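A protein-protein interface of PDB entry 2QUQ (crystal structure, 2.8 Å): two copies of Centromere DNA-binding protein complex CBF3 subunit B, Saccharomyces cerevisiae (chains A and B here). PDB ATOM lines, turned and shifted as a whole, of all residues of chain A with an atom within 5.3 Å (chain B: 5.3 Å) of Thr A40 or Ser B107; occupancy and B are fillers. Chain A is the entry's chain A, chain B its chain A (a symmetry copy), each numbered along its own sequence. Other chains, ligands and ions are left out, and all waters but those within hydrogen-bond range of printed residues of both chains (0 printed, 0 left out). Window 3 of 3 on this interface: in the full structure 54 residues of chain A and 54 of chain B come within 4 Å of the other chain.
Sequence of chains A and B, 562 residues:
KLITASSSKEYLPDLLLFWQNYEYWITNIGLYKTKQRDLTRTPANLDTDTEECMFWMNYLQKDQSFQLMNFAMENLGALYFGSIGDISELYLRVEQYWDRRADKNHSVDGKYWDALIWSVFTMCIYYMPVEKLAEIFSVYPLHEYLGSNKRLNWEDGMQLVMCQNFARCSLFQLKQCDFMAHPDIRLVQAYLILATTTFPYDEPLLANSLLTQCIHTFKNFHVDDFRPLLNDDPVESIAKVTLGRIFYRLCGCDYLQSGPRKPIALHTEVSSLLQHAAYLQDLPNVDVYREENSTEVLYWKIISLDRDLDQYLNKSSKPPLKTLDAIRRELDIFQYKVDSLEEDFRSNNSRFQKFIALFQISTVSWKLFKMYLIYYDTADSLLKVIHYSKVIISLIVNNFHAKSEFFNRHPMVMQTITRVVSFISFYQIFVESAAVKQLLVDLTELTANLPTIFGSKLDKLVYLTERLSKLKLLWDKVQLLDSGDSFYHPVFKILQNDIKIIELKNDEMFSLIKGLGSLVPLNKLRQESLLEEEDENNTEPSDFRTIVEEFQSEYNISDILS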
ATOM      1  N   ASP A  38     -21.022   6.730  -0.339  1.00  0.00           N
ATOM      2  CA  ASP A  38     -21.792   6.327  -1.517  1.00  0.00           C
ATOM      3  C   ASP A  38     -22.088   7.572  -2.345  1.00  0.00           C
ATOM      4  O   ASP A  38     -22.827   8.469  -1.919  1.00  0.00           O
ATOM      5  CB  ASP A  38     -23.099   5.638  -1.119  1.00  0.00           C
ATOM      6  CG  ASP A  38     -23.871   5.138  -2.321  1.00  0.00           C
ATOM      7  OD1 ASP A  38     -24.435   5.976  -3.050  1.00  0.00           O
ATOM      8  OD2 ASP A  38     -23.902   3.912  -2.550  1.00  0.00           O
ATOM      9  N   LEU A  39     -21.501   7.619  -3.533  1.00  0.00           N
ATOM     10  CA  LEU A  39     -21.661   8.767  -4.400  1.00  0.00           C
ATOM     11  C   LEU A  39     -23.053   8.925  -4.977  1.00  0.00           C
ATOM     12  O   LEU A  39     -23.456  10.032  -5.335  1.00  0.00           O
ATOM     13  CB  LEU A  39     -20.611   8.716  -5.509  1.00  0.00           C
ATOM     14  CG  LEU A  39     -19.194   8.881  -4.957  1.00  0.00           C
ATOM     15  CD1 LEU A  39     -18.161   8.784  -6.082  1.00  0.00           C
ATOM     16  CD2 LEU A  39     -19.105  10.220  -4.240  1.00  0.00           C
ATOM     17  N   THR A  40     -23.792   7.826  -5.064  1.00  0.00           N
ATOM     18  CA  THR A  40     -25.151   7.890  -5.583  1.00  0.00           C
ATOM     19  C   THR A  40     -26.029   8.600  -4.542  1.00  0.00           C
ATOM     20  O   THR A  40     -27.056   9.194  -4.875  1.00  0.00           O
ATOM     21  CB  THR A  40     -25.747   6.492  -5.810  1.00  0.00           C
ATOM     22  OG1 THR A  40     -26.475   6.113  -4.637  1.00  0.00           O
ATOM     23  CG2 THR A  40     -24.647   5.453  -6.085  1.00  0.00           C
ATOM     24  N   ARG A  41     -25.607   8.538  -3.281  1.00  0.00           N
ATOM     25  CA  ARG A  41     -26.350   9.147  -2.185  1.00  0.00           C
ATOM     26  C   ARG A  41     -25.808  10.491  -1.721  1.00  0.00           C
ATOM     27  O   ARG A  41     -26.397  11.126  -0.852  1.00  0.00           O
ATOM     28  CB  ARG A  41     -26.376   8.199  -0.989  1.00  0.00           C
ATOM     29  CG  ARG A  41     -26.741   6.793  -1.356  1.00  0.00           C
ATOM     30  CD  ARG A  41     -27.640   6.179  -0.321  1.00  0.00           C
ATOM     31  NE  ARG A  41     -28.220   4.945  -0.829  1.00  0.00           N
ATOM     32  CZ  ARG A  41     -29.268   4.338  -0.289  1.00  0.00           C
ATOM     33  NH1 ARG A  41     -29.852   4.856   0.786  1.00  0.00           N
ATOM     34  NH2 ARG A  41     -29.737   3.219  -0.829  1.00  0.00           N
ATOM     35  N   THR A  42     -24.691  10.932  -2.286  1.00  0.00           N
ATOM     36  CA  THR A  42     -24.117  12.202  -1.859  1.00  0.00           C
ATOM     37  C   THR A  42     -24.582  13.393  -2.681  1.00  0.00           C
ATOM     38  O   THR A  42     -24.387  13.445  -3.888  1.00  0.00           O
ATOM     39  CB  THR A  42     -22.571  12.165  -1.883  1.00  0.00           C
ATOM     40  OG1 THR A  42     -22.095  11.084  -1.064  1.00  0.00           O
ATOM     41  CG2 THR A  42     -22.012  13.482  -1.358  1.00  0.00           C
ATOM     42  N   PRO A  43     -25.208  14.375  -2.027  1.00  0.00           N
ATOM     43  CA  PRO A  43     -25.679  15.552  -2.750  1.00  0.00           C
ATOM     44  C   PRO A  43     -24.476  16.326  -3.259  1.00  0.00           C
ATOM     45  O   PRO A  43     -23.461  16.417  -2.571  1.00  0.00           O
ATOM     46  CB  PRO A  43     -26.452  16.311  -1.685  1.00  0.00           C
ATOM     47  CG  PRO A  43     -25.659  16.018  -0.451  1.00  0.00           C
ATOM     48  CD  PRO A  43     -25.408  14.533  -0.577  1.00  0.00           C
ATOM     49  N   ALA A  44     -24.584  16.878  -4.462  1.00  0.00           N
ATOM     50  CA  ALA A  44     -23.482  17.632  -5.041  1.00  0.00           C
ATOM     51  C   ALA A  44     -23.970  18.973  -5.550  1.00  0.00           C
ATOM     52  O   ALA A  44     -25.128  19.098  -5.920  1.00  0.00           O
ATOM     53  CB  ALA A  44     -22.865  16.839  -6.182  1.00  0.00           C
ATOM     54  N   ASN B 105     -32.764  18.271  -7.429  1.00  0.00           N
ATOM     55  CA  ASN B 105     -32.048  17.338  -6.588  1.00  0.00           C
ATOM     56  C   ASN B 105     -31.057  16.563  -7.452  1.00  0.00           C
ATOM     57  O   ASN B 105     -31.454  15.755  -8.290  1.00  0.00           O
ATOM     58  CB  ASN B 105     -33.049  16.387  -5.914  1.00  0.00           C
ATOM     59  CG  ASN B 105     -34.226  16.020  -6.825  1.00  0.00           C
ATOM     60  OD1 ASN B 105     -34.991  16.885  -7.261  1.00  0.00           O
ATOM     61  ND2 ASN B 105     -34.374  14.730  -7.107  1.00  0.00           N
ATOM     62  N   HIS B 106     -29.767  16.826  -7.255  1.00  0.00           N
ATOM     63  CA  HIS B 106     -28.727  16.147  -8.024  1.00  0.00           C
ATOM     64  C   HIS B 106     -27.571  15.655  -7.148  1.00  0.00           C
ATOM     65  O   HIS B 106     -27.063  16.393  -6.303  1.00  0.00           O
ATOM     66  CB  HIS B 106     -28.218  17.077  -9.130  1.00  0.00           C
ATOM     67  CG  HIS B 106     -28.533  16.593 -10.511  1.00  0.00           C
ATOM     68  ND1 HIS B 106     -28.646  17.441 -11.590  1.00  0.00           N
ATOM     69  CD2 HIS B 106     -28.726  15.341 -10.995  1.00  0.00           C
ATOM     70  CE1 HIS B 106     -28.893  16.734 -12.679  1.00  0.00           C
ATOM     71  NE2 HIS B 106     -28.946  15.457 -12.345  1.00  0.00           N
ATOM     72  N   SER B 107     -27.163  14.405  -7.366  1.00  0.00           N
ATOM     73  CA  SER B 107     -26.094  13.781  -6.586  1.00  0.00           C
ATOM     74  C   SER B 107     -24.673  14.010  -7.101  1.00  0.00           C
ATOM     75  O   SER B 107     -24.381  15.006  -7.764  1.00  0.00           O
ATOM     76  CB  SER B 107     -26.347  12.267  -6.465  1.00  0.00           C
ATOM     77  OG  SER B 107     -26.172  11.580  -7.694  1.00  0.00           O
ATOM     78  N   VAL B 108     -23.789  13.074  -6.765  1.00  0.00           N
ATOM     79  CA  VAL B 108     -22.399  13.136  -7.174  1.00  0.00           C
ATOM     80  C   VAL B 108     -22.185  12.078  -8.230  1.00  0.00           C
ATOM     81  O   VAL B 108     -21.593  12.349  -9.270  1.00  0.00           O
ATOM     82  CB  VAL B 108     -21.447  12.890  -5.981  1.00  0.00           C
ATOM     83  CG1 VAL B 108     -20.010  12.811  -6.454  1.00  0.00           C
ATOM     84  CG2 VAL B 108     -21.582  14.019  -4.986  1.00  0.00           C
ATOM     85  N   ASP B 109     -22.669  10.868  -7.984  1.00  0.00           N
ATOM     86  CA  ASP B 109     -22.503   9.837  -8.994  1.00  0.00           C
ATOM     87  C   ASP B 109     -23.227  10.371 -10.206  1.00  0.00           C
ATOM     88  O   ASP B 109     -22.932  10.000 -11.344  1.00  0.00           O
ATOM     89  CB  ASP B 109     -23.125   8.510  -8.579  1.00  0.00           C
ATOM     90  CG  ASP B 109     -22.892   7.425  -9.615  1.00  0.00           C
ATOM     91  OD1 ASP B 109     -21.727   7.256 -10.027  1.00  0.00           O
ATOM     92  OD2 ASP B 109     -23.857   6.744 -10.027  1.00  0.00           O
ATOM     93  N   GLY B 110     -24.180  11.256  -9.941  1.00  0.00           N
ATOM     94  CA  GLY B 110     -24.944  11.863 -11.008  1.00  0.00           C
ATOM     95  C   GLY B 110     -24.029  12.723 -11.851  1.00  0.00           C
ATOM     96  O   GLY B 110     -23.770  12.404 -13.008  1.00  0.00           O
ATOM     97  N   LYS B 111     -23.528  13.808 -11.269  1.00  0.00           N
ATOM     98  CA  LYS B 111     -22.635  14.714 -11.975  1.00  0.00           C
ATOM     99  C   LYS B 111     -21.458  14.004 -12.644  1.00  0.00           C
ATOM    100  O   LYS B 111     -21.177  14.253 -13.813  1.00  0.00           O
ATOM    101  CB  LYS B 111     -22.130  15.795 -11.019  1.00  0.00           C
ATOM    102  CG  LYS B 111     -23.191  16.820 -10.676  1.00  0.00           C
ATOM    103  CD  LYS B 111     -23.643  17.521 -11.947  1.00  0.00           C
ATOM    104  CE  LYS B 111     -24.936  18.284 -11.750  1.00  0.00           C
ATOM    105  NZ  LYS B 111     -25.305  19.045 -12.973  1.00  0.00           N
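Ser B107 touches Leu A39.
Thr A40 touches Ser B107 (O to CB, 3.5 Å).
N of Thr A40 touches CB of Asp B109 (3.6 Å).
O of Thr A42 touches CA of Ser B107, at 3.2 Å.
Pro A43 touches His B106 (CA to O, 3.9 Å).
Val B108 touches Pro A43.
Ala A44 touches Ser B107 (CB to O, 2.9 Å).
Ala A44 touches Val B108.
Thr A40 touches just these residues of chain B: Ser B107 (3.5 Å) and Asp B109 (3.6 Å).
Ser B107 touches just these residues of chain A: Leu A39 (3.8 Å), Thr A40 (3.5 Å), Thr A42 (3.2 Å) and Ala A44 (2.9 Å).
Of the printed residues of chain B, Pro A43 touches His B106 (3.9 Å) and Val B108 (3.9 Å).
Of the printed residues of chain B, Ala A44 touches His B106 (3.1 Å), Ser B107 (2.9 Å) and Val B108 (3.3 Å).
Of the printed residues of chain B, Thr A42 touches Ser B107 (3.2 Å) and Val B108 (3.0 Å).
Gly B110 touches none of the printed residues of chain A.
The nearest printed residue of chain B that does not touch Thr A40 is Val B108 (5.4 Å).
Hydrophobic or aromatic side chains of chain B that line the printed part of chain A: Val B108.
Hydrophobic or aromatic side chains of chain A within 4 Å of the printed part of chain B: Leu A39 and Ala A44.
Among the printed residues, 12 pairs touch across the chains.
No position is printed for both chains.
O of Leu A39 lies within hydrogen-bond range of N of Val B108.
N of Asp B109 is in hydrogen-bond range of O of Leu A39 (2.9 Å).
The backbone carbonyl oxygen (O) of Thr A42 lies within hydrogen-bond range of the backbone NH (N) of Val B108, at 3.0 Å.
O of His B106 lies within hydrogen-bond range of N of Ala A44, 3.1 Å away.
The side-chain hydroxyl (OG1) of Thr A40 sits at hydrogen-bond distance from the side-chain carboxylate (OD1) of Asp A38 (2.6 Å).
OG1 of Thr A42 lies within hydrogen-bond range of O of Asp A38 (2.8 Å).
The side-chain hydroxyl (OG) of Ser B107 is in hydrogen-bond range of the backbone NH (N) of Gly B110, 3.0 Å away.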
